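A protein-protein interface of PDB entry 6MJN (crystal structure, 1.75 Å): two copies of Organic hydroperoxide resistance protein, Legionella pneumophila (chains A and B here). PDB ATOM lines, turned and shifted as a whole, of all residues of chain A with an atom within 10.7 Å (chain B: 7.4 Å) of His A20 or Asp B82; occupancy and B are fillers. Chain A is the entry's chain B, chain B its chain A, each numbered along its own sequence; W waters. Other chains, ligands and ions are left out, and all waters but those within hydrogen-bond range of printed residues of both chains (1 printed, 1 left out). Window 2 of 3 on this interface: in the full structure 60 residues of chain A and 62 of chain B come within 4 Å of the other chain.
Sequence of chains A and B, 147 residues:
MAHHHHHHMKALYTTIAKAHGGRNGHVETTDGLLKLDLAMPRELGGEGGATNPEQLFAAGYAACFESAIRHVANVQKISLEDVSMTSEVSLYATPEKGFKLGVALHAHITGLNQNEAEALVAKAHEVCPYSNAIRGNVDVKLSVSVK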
ATOM      1  N   ALA A  17       6.909 -26.924 -19.949  1.00  0.00           N
ATOM      2  CA  ALA A  17       7.841 -25.804 -19.809  1.00  0.00           C
ATOM      3  C   ALA A  17       7.210 -24.517 -20.308  1.00  0.00           C
ATOM      4  O   ALA A  17       6.419 -24.529 -21.254  1.00  0.00           O
ATOM      5  CB  ALA A  17       9.132 -26.028 -20.587  1.00  0.00           C
ATOM      6  N   LYS A  18       7.580 -23.394 -19.683  1.00  0.00           N
ATOM      7  CA  LYS A  18       7.043 -22.085 -20.052  1.00  0.00           C
ATOM      8  C   LYS A  18       8.217 -21.132 -20.215  1.00  0.00           C
ATOM      9  O   LYS A  18       9.072 -21.044 -19.322  1.00  0.00           O
ATOM     10  CB  LYS A  18       6.058 -21.568 -19.009  1.00  0.00           C
ATOM     11  CG  LYS A  18       4.794 -22.418 -18.840  1.00  0.00           C
ATOM     12  CD  LYS A  18       3.868 -21.813 -17.802  1.00  0.00           C
ATOM     13  CE  LYS A  18       2.514 -22.506 -17.808  1.00  0.00           C
ATOM     14  NZ  LYS A  18       1.557 -21.853 -16.867  1.00  0.00           N
ATOM     15  N   ALA A  19       8.315 -20.512 -21.393  1.00  0.00           N
ATOM     16  CA  ALA A  19       9.389 -19.583 -21.719  1.00  0.00           C
ATOM     17  C   ALA A  19       8.807 -18.196 -21.934  1.00  0.00           C
ATOM     18  O   ALA A  19       7.695 -18.049 -22.442  1.00  0.00           O
ATOM     19  CB  ALA A  19      10.158 -20.022 -22.979  1.00  0.00           C
ATOM     20  N   HIS A  20       9.574 -17.173 -21.540  1.00  0.00           N
ATOM     21  CA  HIS A  20       9.160 -15.787 -21.710  1.00  0.00           C
ATOM     22  C   HIS A  20      10.406 -14.915 -21.773  1.00  0.00           C
ATOM     23  O   HIS A  20      11.488 -15.316 -21.339  1.00  0.00           O
ATOM     24  CB  HIS A  20       8.236 -15.318 -20.572  1.00  0.00           C
ATOM     25  CG  HIS A  20       7.816 -13.882 -20.674  1.00  0.00           C
ATOM     26  ND1 HIS A  20       8.250 -12.916 -19.789  1.00  0.00           N
ATOM     27  CD2 HIS A  20       7.000 -13.248 -21.550  1.00  0.00           C
ATOM     28  CE1 HIS A  20       7.719 -11.752 -20.116  1.00  0.00           C
ATOM     29  NE2 HIS A  20       6.950 -11.928 -21.177  1.00  0.00           N
ATOM     30  N   GLY A  21      10.241 -13.722 -22.323  1.00  0.00           N
ATOM     31  CA  GLY A  21      11.321 -12.757 -22.350  1.00  0.00           C
ATOM     32  C   GLY A  21      12.248 -12.842 -23.541  1.00  0.00           C
ATOM     33  O   GLY A  21      13.271 -12.145 -23.554  1.00  0.00           O
ATOM     34  N   GLY A  22      11.936 -13.673 -24.533  1.00  0.00           N
ATOM     35  CA  GLY A  22      12.748 -13.729 -25.733  1.00  0.00           C
ATOM     36  C   GLY A  22      14.052 -14.492 -25.559  1.00  0.00           C
ATOM     37  O   GLY A  22      14.245 -15.284 -24.620  1.00  0.00           O
ATOM     38  N   ARG A  23      14.970 -14.239 -26.503  1.00  0.00           N
ATOM     39  CA  ARG A  23      16.228 -14.981 -26.559  1.00  0.00           C
ATOM     40  C   ARG A  23      17.101 -14.720 -25.339  1.00  0.00           C
ATOM     41  O   ARG A  23      17.943 -15.557 -24.989  1.00  0.00           O
ATOM     42  CB  ARG A  23      16.992 -14.623 -27.834  1.00  0.00           C
ATOM     43  N   ASN A  24      16.933 -13.566 -24.696  1.00  0.00           N
ATOM     44  CA  ASN A  24      17.594 -13.277 -23.435  1.00  0.00           C
ATOM     45  C   ASN A  24      16.670 -13.498 -22.246  1.00  0.00           C
ATOM     46  O   ASN A  24      16.906 -12.938 -21.165  1.00  0.00           O
ATOM     47  CB  ASN A  24      18.136 -11.847 -23.441  1.00  0.00           C
ATOM     48  CG  ASN A  24      19.226 -11.651 -24.477  1.00  0.00           C
ATOM     49  OD1 ASN A  24      20.016 -12.560 -24.739  1.00  0.00           O
ATOM     50  ND2 ASN A  24      19.273 -10.467 -25.074  1.00  0.00           N
ATOM     51  N   GLY A  25      15.646 -14.336 -22.415  1.00  0.00           N
ATOM     52  CA  GLY A  25      14.647 -14.537 -21.390  1.00  0.00           C
ATOM     53  C   GLY A  25      14.936 -15.675 -20.433  1.00  0.00           C
ATOM     54  O   GLY A  25      16.060 -15.830 -19.933  1.00  0.00           O
ATOM     55  N   HIS A  26      13.909 -16.481 -20.184  1.00  0.00           N
ATOM     56  CA  HIS A  26      13.897 -17.435 -19.089  1.00  0.00           C
ATOM     57  C   HIS A  26      12.921 -18.551 -19.441  1.00  0.00           C
ATOM     58  O   HIS A  26      11.899 -18.308 -20.085  1.00  0.00           O
ATOM     59  CB  HIS A  26      13.482 -16.740 -17.787  1.00  0.00           C
ATOM     60  CG  HIS A  26      13.640 -17.590 -16.572  1.00  0.00           C
ATOM     61  ND1 HIS A  26      14.800 -17.609 -15.826  1.00  0.00           N
ATOM     62  CD2 HIS A  26      12.789 -18.453 -15.970  1.00  0.00           C
ATOM     63  CE1 HIS A  26      14.656 -18.449 -14.817  1.00  0.00           C
ATOM     64  NE2 HIS A  26      13.447 -18.977 -14.886  1.00  0.00           N
ATOM     65  N   VAL A  27      13.236 -19.775 -19.018  1.00  0.00           N
ATOM     66  CA  VAL A  27      12.339 -20.913 -19.227  1.00  0.00           C
ATOM     67  C   VAL A  27      12.390 -21.825 -18.007  1.00  0.00           C
ATOM     68  O   VAL A  27      13.466 -22.054 -17.438  1.00  0.00           O
ATOM     69  CB  VAL A  27      12.697 -21.676 -20.527  1.00  0.00           C
ATOM     70  CG1 VAL A  27      14.111 -22.249 -20.444  1.00  0.00           C
ATOM     71  CG2 VAL A  27      11.680 -22.768 -20.831  1.00  0.00           C
ATOM     72  N   GLU A  28      11.219 -22.331 -17.587  1.00  0.00           N
ATOM     73  CA  GLU A  28      11.119 -23.195 -16.406  1.00  0.00           C
ATOM     74  C   GLU A  28      10.136 -24.320 -16.676  1.00  0.00           C
ATOM     75  O   GLU A  28       9.131 -24.122 -17.364  1.00  0.00           O
ATOM     76  CB  GLU A  28      10.612 -22.461 -15.138  1.00  0.00           C
ATOM     77  CG  GLU A  28      11.559 -21.424 -14.559  1.00  0.00           C
ATOM     78  CD  GLU A  28      11.099 -20.801 -13.227  1.00  0.00           C
ATOM     79  OE1 GLU A  28      10.157 -21.305 -12.566  1.00  0.00           O
ATOM     80  OE2 GLU A  28      11.709 -19.782 -12.841  1.00  0.00           O
ATOM     81  N   THR A  29      10.384 -25.473 -16.064  1.00  0.00           N
ATOM     82  CA  THR A  29       9.374 -26.514 -16.040  1.00  0.00           C
ATOM     83  C   THR A  29       8.412 -26.231 -14.906  1.00  0.00           C
ATOM     84  O   THR A  29       8.780 -25.624 -13.900  1.00  0.00           O
ATOM     85  CB  THR A  29       9.973 -27.910 -15.859  1.00  0.00           C
ATOM     86  OG1 THR A  29      10.832 -27.942 -14.703  1.00  0.00           O
ATOM     87  CG2 THR A  29      10.755 -28.321 -17.102  1.00  0.00           C
ATOM     88  N   LEU A  36      15.986 -21.938 -16.008  1.00  0.00           N
ATOM     89  CA  LEU A  36      17.138 -21.572 -16.832  1.00  0.00           C
ATOM     90  C   LEU A  36      17.008 -20.172 -17.414  1.00  0.00           C
ATOM     91  O   LEU A  36      15.996 -19.851 -18.039  1.00  0.00           O
ATOM     92  CB  LEU A  36      17.321 -22.558 -17.986  1.00  0.00           C
ATOM     93  CG  LEU A  36      17.652 -24.007 -17.675  1.00  0.00           C
ATOM     94  CD1 LEU A  36      17.598 -24.760 -18.983  1.00  0.00           C
ATOM     95  CD2 LEU A  36      19.020 -24.099 -17.035  1.00  0.00           C
ATOM     96  N   ASP A  37      18.045 -19.356 -17.229  1.00  0.00           N
ATOM     97  CA  ASP A  37      18.195 -18.128 -17.998  1.00  0.00           C
ATOM     98  C   ASP A  37      18.716 -18.464 -19.387  1.00  0.00           C
ATOM     99  O   ASP A  37      19.439 -19.444 -19.570  1.00  0.00           O
ATOM    100  CB  ASP A  37      19.166 -17.168 -17.316  1.00  0.00           C
ATOM    101  CG  ASP A  37      18.582 -16.508 -16.078  1.00  0.00           C
ATOM    102  OD1 ASP A  37      17.343 -16.458 -15.935  1.00  0.00           O
ATOM    103  OD2 ASP A  37      19.373 -16.012 -15.249  1.00  0.00           O
ATOM    104  N   LEU A  38      18.362 -17.628 -20.359  1.00  0.00           N
ATOM    105  CA  LEU A  38      18.707 -17.824 -21.755  1.00  0.00           C
ATOM    106  C   LEU A  38      19.464 -16.609 -22.272  1.00  0.00           C
ATOM    107  O   LEU A  38      19.274 -15.492 -21.793  1.00  0.00           O
ATOM    108  CB  LEU A  38      17.451 -18.026 -22.609  1.00  0.00           C
ATOM    109  CG  LEU A  38      16.537 -19.154 -22.153  1.00  0.00           C
ATOM    110  CD1 LEU A  38      15.172 -19.079 -22.821  1.00  0.00           C
ATOM    111  CD2 LEU A  38      17.243 -20.453 -22.497  1.00  0.00           C
ATOM    112  N   ALA A  39      20.309 -16.825 -23.275  1.00  0.00           N
ATOM    113  CA  ALA A  39      20.926 -15.702 -23.966  1.00  0.00           C
ATOM    114  C   ALA A  39      21.305 -16.133 -25.370  1.00  0.00           C
ATOM    115  O   ALA A  39      21.662 -17.287 -25.606  1.00  0.00           O
ATOM    116  CB  ALA A  39      22.161 -15.175 -23.223  1.00  0.00           C
ATOM    117  N   THR A  51      22.554 -20.268 -21.321  1.00  0.00           N
ATOM    118  CA  THR A  51      22.353 -21.327 -22.307  1.00  0.00           C
ATOM    119  C   THR A  51      21.335 -20.895 -23.366  1.00  0.00           C
ATOM    120  O   THR A  51      20.841 -19.763 -23.370  1.00  0.00           O
ATOM    121  CB  THR A  51      21.936 -22.629 -21.622  1.00  0.00           C
ATOM    122  OG1 THR A  51      22.076 -23.726 -22.546  1.00  0.00           O
ATOM    123  CG2 THR A  51      20.501 -22.565 -21.165  1.00  0.00           C
ATOM    124  N   PRO A  53      18.553 -22.772 -26.811  1.00  0.00           N
ATOM    125  CA  PRO A  53      17.913 -24.018 -27.273  1.00  0.00           C
ATOM    126  C   PRO A  53      18.851 -25.025 -27.936  1.00  0.00           C
ATOM    127  O   PRO A  53      18.563 -26.220 -27.854  1.00  0.00           O
ATOM    128  CB  PRO A  53      16.849 -23.516 -28.264  1.00  0.00           C
ATOM    129  CG  PRO A  53      16.504 -22.143 -27.743  1.00  0.00           C
ATOM    130  CD  PRO A  53      17.828 -21.579 -27.298  1.00  0.00           C
ATOM    131  N   ALA B  62      10.043 -24.667 -26.186  1.00  0.00           N
ATOM    132  CA  ALA B  62       9.271 -23.475 -25.799  1.00  0.00           C
ATOM    133  C   ALA B  62      10.056 -22.203 -26.090  1.00  0.00           C
ATOM    134  O   ALA B  62       9.504 -21.222 -26.604  1.00  0.00           O
ATOM    135  CB  ALA B  62       8.893 -23.525 -24.314  1.00  0.00           C
ATOM    136  N   ALA B  63      11.347 -22.203 -25.765  1.00  0.00           N
ATOM    137  CA  ALA B  63      12.169 -21.024 -26.032  1.00  0.00           C
ATOM    138  C   ALA B  63      12.382 -20.836 -27.532  1.00  0.00           C
ATOM    139  O   ALA B  63      12.307 -19.711 -28.043  1.00  0.00           O
ATOM    140  CB  ALA B  63      13.512 -21.158 -25.302  1.00  0.00           C
ATOM    141  N   GLU B  66       9.178 -19.527 -29.191  1.00  0.00           N
ATOM    142  CA  GLU B  66       8.939 -18.128 -28.859  1.00  0.00           C
ATOM    143  C   GLU B  66       9.849 -17.206 -29.665  1.00  0.00           C
ATOM    144  O   GLU B  66       9.424 -16.134 -30.115  1.00  0.00           O
ATOM    145  CB  GLU B  66       9.136 -17.873 -27.350  1.00  0.00           C
ATOM    146  CG  GLU B  66       8.755 -16.452 -26.937  1.00  0.00           C
ATOM    147  CD  GLU B  66       9.419 -16.000 -25.646  1.00  0.00           C
ATOM    148  OE1 GLU B  66       9.874 -16.871 -24.876  1.00  0.00           O
ATOM    149  OE2 GLU B  66       9.480 -14.772 -25.407  1.00  0.00           O
ATOM    150  N   ILE B  69       8.467 -16.903 -33.230  1.00  0.00           N
ATOM    151  CA  ILE B  69       7.365 -15.947 -33.310  1.00  0.00           C
ATOM    152  C   ILE B  69       7.897 -14.514 -33.399  1.00  0.00           C
ATOM    153  O   ILE B  69       7.499 -13.729 -34.273  1.00  0.00           O
ATOM    154  CB  ILE B  69       6.418 -16.122 -32.110  1.00  0.00           C
ATOM    155  CG1 ILE B  69       5.685 -17.468 -32.191  1.00  0.00           C
ATOM    156  CG2 ILE B  69       5.421 -14.951 -32.076  1.00  0.00           C
ATOM    157  CD1 ILE B  69       4.863 -17.808 -30.948  1.00  0.00           C
ATOM    158  N   ARG B  70       8.811 -14.146 -32.493  1.00  0.00           N
ATOM    159  CA  ARG B  70       9.332 -12.781 -32.506  1.00  0.00           C
ATOM    160  C   ARG B  70      10.119 -12.485 -33.780  1.00  0.00           C
ATOM    161  O   ARG B  70      10.086 -11.351 -34.282  1.00  0.00           O
ATOM    162  CB  ARG B  70      10.194 -12.543 -31.266  1.00  0.00           C
ATOM    163  CG  ARG B  70       9.460 -12.736 -29.947  1.00  0.00           C
ATOM    164  CD  ARG B  70      10.346 -12.349 -28.769  1.00  0.00           C
ATOM    165  NE  ARG B  70       9.745 -12.572 -27.452  1.00  0.00           N
ATOM    166  CZ  ARG B  70       9.043 -11.658 -26.784  1.00  0.00           C
ATOM    167  NH1 ARG B  70       8.833 -10.465 -27.324  1.00  0.00           N
ATOM    168  NH2 ARG B  70       8.548 -11.927 -25.577  1.00  0.00           N
ATOM    169  N   SER B  79       3.752  -5.497 -34.934  1.00  0.00           N
ATOM    170  CA  SER B  79       4.043  -5.043 -33.577  1.00  0.00           C
ATOM    171  C   SER B  79       3.410  -5.992 -32.566  1.00  0.00           C
ATOM    172  O   SER B  79       2.180  -6.121 -32.509  1.00  0.00           O
ATOM    173  CB  SER B  79       3.536  -3.617 -33.360  1.00  0.00           C
ATOM    174  OG  SER B  79       4.412  -2.660 -33.933  1.00  0.00           O
ATOM    175  N   LEU B  80       4.254  -6.645 -31.769  1.00  0.00           N
ATOM    176  CA  LEU B  80       3.840  -7.567 -30.719  1.00  0.00           C
ATOM    177  C   LEU B  80       4.003  -6.886 -29.374  1.00  0.00           C
ATOM    178  O   LEU B  80       5.078  -6.356 -29.073  1.00  0.00           O
ATOM    179  CB  LEU B  80       4.691  -8.841 -30.733  1.00  0.00           C
ATOM    180  CG  LEU B  80       4.473  -9.935 -31.762  1.00  0.00           C
ATOM    181  CD1 LEU B  80       5.563 -11.027 -31.615  1.00  0.00           C
ATOM    182  CD2 LEU B  80       3.103 -10.527 -31.552  1.00  0.00           C
ATOM    183  N   GLU B  81       2.956  -6.902 -28.557  1.00  0.00           N
ATOM    184  CA  GLU B  81       3.153  -6.348 -27.227  1.00  0.00           C
ATOM    185  C   GLU B  81       3.834  -7.352 -26.315  1.00  0.00           C
ATOM    186  O   GLU B  81       4.618  -6.958 -25.446  1.00  0.00           O
ATOM    187  CB  GLU B  81       1.831  -5.867 -26.636  1.00  0.00           C
ATOM    188  CG  GLU B  81       1.511  -4.428 -27.027  1.00  0.00           C
ATOM    189  CD  GLU B  81       0.038  -4.093 -26.915  1.00  0.00           C
ATOM    190  OE1 GLU B  81      -0.721  -4.915 -26.362  1.00  0.00           O
ATOM    191  OE2 GLU B  81      -0.357  -3.004 -27.385  1.00  0.00           O
ATOM    192  N   ASP B  82       3.580  -8.639 -26.511  1.00  0.00           N
ATOM    193  CA  ASP B  82       4.199  -9.651 -25.667  1.00  0.00           C
ATOM    194  C   ASP B  82       3.917 -11.020 -26.262  1.00  0.00           C
ATOM    195  O   ASP B  82       2.973 -11.199 -27.036  1.00  0.00           O
ATOM    196  CB  ASP B  82       3.689  -9.568 -24.220  1.00  0.00           C
ATOM    197  CG  ASP B  82       4.651 -10.191 -23.223  1.00  0.00           C
ATOM    198  OD1 ASP B  82       5.771 -10.580 -23.626  1.00  0.00           O
ATOM    199  OD2 ASP B  82       4.283 -10.288 -22.031  1.00  0.00           O
ATOM    200  N   VAL B  83       4.785 -11.971 -25.924  1.00  0.00           N
ATOM    201  CA  VAL B  83       4.627 -13.377 -26.276  1.00  0.00           C
ATOM    202  C   VAL B  83       5.167 -14.205 -25.124  1.00  0.00           C
ATOM    203  O   VAL B  83       6.217 -13.886 -24.559  1.00  0.00           O
ATOM    204  CB  VAL B  83       5.382 -13.764 -27.570  1.00  0.00           C
ATOM    205  CG1 VAL B  83       5.009 -15.176 -28.002  1.00  0.00           C
ATOM    206  CG2 VAL B  83       5.142 -12.762 -28.680  1.00  0.00           C
ATOM    207  N   SER B  84       4.455 -15.266 -24.774  1.00  0.00           N
ATOM    208  CA  SER B  84       5.028 -16.319 -23.951  1.00  0.00           C
ATOM    209  C   SER B  84       4.611 -17.648 -24.565  1.00  0.00           C
ATOM    210  O   SER B  84       3.637 -17.728 -25.315  1.00  0.00           O
ATOM    211  CB  SER B  84       4.595 -16.204 -22.484  1.00  0.00           C
ATOM    212  OG  SER B  84       3.220 -16.466 -22.348  1.00  0.00           O
ATOM    213  N   MET B  85       5.384 -18.685 -24.276  1.00  0.00           N
ATOM    214  CA  MET B  85       5.235 -19.964 -24.935  1.00  0.00           C
ATOM    215  C   MET B  85       5.214 -21.086 -23.906  1.00  0.00           C
ATOM    216  O   MET B  85       6.107 -21.169 -23.059  1.00  0.00           O
ATOM    217  CB  MET B  85       6.396 -20.136 -25.899  1.00  0.00           C
ATOM    218  CG  MET B  85       6.169 -21.158 -26.956  1.00  0.00           C
ATOM    219  SD  MET B  85       4.841 -20.677 -28.072  1.00  0.00           S
ATOM    220  CE  MET B  85       4.293 -22.335 -28.330  1.00  0.00           C
ATOM    221  N   HIS B 108       0.917 -17.668 -26.262  1.00  0.00           N
ATOM    222  CA  HIS B 108       0.085 -16.618 -25.669  1.00  0.00           C
ATOM    223  C   HIS B 108       0.615 -15.290 -26.187  1.00  0.00           C
ATOM    224  O   HIS B 108       1.758 -14.917 -25.898  1.00  0.00           O
ATOM    225  CB  HIS B 108       0.150 -16.645 -24.144  1.00  0.00           C
ATOM    226  CG  HIS B 108      -0.311 -17.931 -23.539  1.00  0.00           C
ATOM    227  ND1 HIS B 108      -1.581 -18.098 -23.030  1.00  0.00           N
ATOM    228  CD2 HIS B 108       0.334 -19.106 -23.341  1.00  0.00           C
ATOM    229  CE1 HIS B 108      -1.702 -19.325 -22.553  1.00  0.00           C
ATOM    230  NE2 HIS B 108      -0.556 -19.958 -22.731  1.00  0.00           N
ATOM    231  N   ILE B 109      -0.190 -14.585 -26.964  1.00  0.00           N
ATOM    232  CA  ILE B 109       0.282 -13.415 -27.694  1.00  0.00           C
ATOM    233  C   ILE B 109      -0.579 -12.232 -27.318  1.00  0.00           C
ATOM    234  O   ILE B 109      -1.807 -12.338 -27.290  1.00  0.00           O
ATOM    235  CB  ILE B 109       0.248 -13.655 -29.217  1.00  0.00           C
ATOM    236  CG1 ILE B 109       1.426 -14.530 -29.640  1.00  0.00           C
ATOM    237  CG2 ILE B 109       0.278 -12.323 -29.975  1.00  0.00           C
ATOM    238  CD1 ILE B 109       1.287 -15.047 -31.068  1.00  0.00           C
ATOM    239  N   THR B 110       0.060 -11.113 -27.012  1.00  0.00           N
ATOM    240  CA  THR B 110      -0.634  -9.885 -26.683  1.00  0.00           C
ATOM    241  C   THR B 110      -0.494  -8.910 -27.845  1.00  0.00           C
ATOM    242  O   THR B 110       0.616  -8.704 -28.348  1.00  0.00           O
ATOM    243  CB  THR B 110      -0.049  -9.293 -25.405  1.00  0.00           C
ATOM    244  OG1 THR B 110      -0.002 -10.317 -24.408  1.00  0.00           O
ATOM    245  CG2 THR B 110      -0.889  -8.162 -24.914  1.00  0.00           C
ATOM    246  N   GLY B 111      -1.615  -8.334 -28.275  1.00  0.00           N
ATOM    247  CA  GLY B 111      -1.613  -7.234 -29.227  1.00  0.00           C
ATOM    248  C   GLY B 111      -2.090  -7.575 -30.623  1.00  0.00           C
ATOM    249  O   GLY B 111      -2.088  -6.690 -31.486  1.00  0.00           O
ATOM    250  N   LEU B 112      -2.510  -8.817 -30.873  1.00  0.00           N
ATOM    251  CA  LEU B 112      -3.019  -9.248 -32.166  1.00  0.00           C
ATOM    252  C   LEU B 112      -4.369  -9.917 -31.964  1.00  0.00           C
ATOM    253  O   LEU B 112      -4.597 -10.573 -30.946  1.00  0.00           O
ATOM    254  CB  LEU B 112      -2.066 -10.240 -32.838  1.00  0.00           C
ATOM    255  CG  LEU B 112      -0.650  -9.737 -33.111  1.00  0.00           C
ATOM    256  CD1 LEU B 112       0.188 -10.894 -33.678  1.00  0.00           C
ATOM    257  CD2 LEU B 112      -0.718  -8.633 -34.109  1.00  0.00           C
HETATM  258  O   HOH W   1      13.311 -17.314 -26.664  1.00  0.00           O
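Among the printed residues, merely in contact across the chains: Ala A17 with Met B85 (3.8 Å), Lys A18 with Met B85 (3.3 Å), Ala A19 with Ala B62 (3.8 Å), Ala A19 with Ala B63 (3.7 Å), Ala A19 with Ser B84 (3.5 Å), His A20 with Val B83 (3.2 Å), His A20 with Ser B84 (3.9 Å), Gly A22 with Arg B70 (3.6 Å), Leu A38 with Ala B63 (3.6 Å) and Pro A53 with Ala B63 (3.99 Å).
Water W1 lies within hydrogen-bond range of O of Ala B63 (2.9 Å), O of Gly A22 (3.0 Å) and N of Arg A23 (3.5 Å).
The backbone NH (N) of Thr B110 sits at hydrogen-bond distance from the backbone carbonyl oxygen (O) of Asp B82 (2.9 Å).
The backbone carbonyl oxygen (O) of His A20 is in hydrogen-bond range of the backbone NH (N) of His A26 (2.9 Å).
The guanidinium group of Arg B70 lies within hydrogen-bond range of the backbone carbonyl oxygen of Val B83 (3.2 Å).
N of Lys A18 sits at hydrogen-bond distance from O of Glu A28 (2.9 Å).
The backbone NH (N) of Leu A38 is in hydrogen-bond range of the backbone carbonyl oxygen (O) of Gly A25 (3.0 Å).
OD1 of Asp B82 lies within salt-bridge range of NH2 of Arg B70 (3.7 Å).
Of the printed residues of chain B, His A20 touches Glu B66 (3.4 Å), Asp B82 (3.0 Å), Val B83 (3.2 Å) and Ser B84 (3.9 Å).
Of the printed residues of chain A, Asp B82 touches His A20.
No residue of chain A comes within 4 Å of Leu B80.
No residue of chain A comes within 4 Å of Thr B110.
Printed residues of chain B within 4 Å of Ala A17: Met B85 (3.8 Å).
Printed residues of chain A within 4 Å of Arg B70: Gly A22 (3.6 Å).
Of the printed residues of chain B, Pro A53 touches Ala B63 (3.99 Å).
The nearest printed residue of chain B that does not touch His A20 is Arg B70 (4.5 Å).
The nearest printed residue of chain A that does not touch Met B85 is His A20 (5.2 Å).
Of the 19 printed residues of chain A, 8 touch a printed residue of chain B.
Printed residues of chain B that touch a printed residue of chain A: Ala B62, Ala B63, Glu B66, Arg B70, Asp B82, Val B83, Ser B84 and Met B85.
Hydrophobic or aromatic side chains of chain B within 4 Å of the printed part of chain A: Ala B62 and Ala B63.
Among the printed residues, no Asp or Glu carboxylate lies within 4 Å of a Lys or Arg side-chain nitrogen of the other chain.
The side-chain carboxylate of Asp B82 lies within hydrogen-bond range of a ring nitrogen (NE2) of His A20.
The backbone NH (N) of Gly A21 is in hydrogen-bond range of the side-chain carboxylate (OE2) of Glu B66, at 3.3 Å.
The side-chain carboxylate of Glu B66 sits at hydrogen-bond distance from the backbone NH of His A20 (3.4 Å).
The backbone carbonyl oxygen (O) of Ala A19 lies close to the side-chain carboxylate (OE1) of Glu B66 (3.5 Å).
O of Met B85 lies within hydrogen-bond range of N of Ala A19 (2.8 Å).
The side-chain carboxylate of Glu B66 lies within hydrogen-bond range of the backbone NH of Gly A22, 2.8 Å away.
No position is printed for both chains.
Of the 16 pairs that touch across the chains among the printed residues, none has its exchanged pair printed and touching as well.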
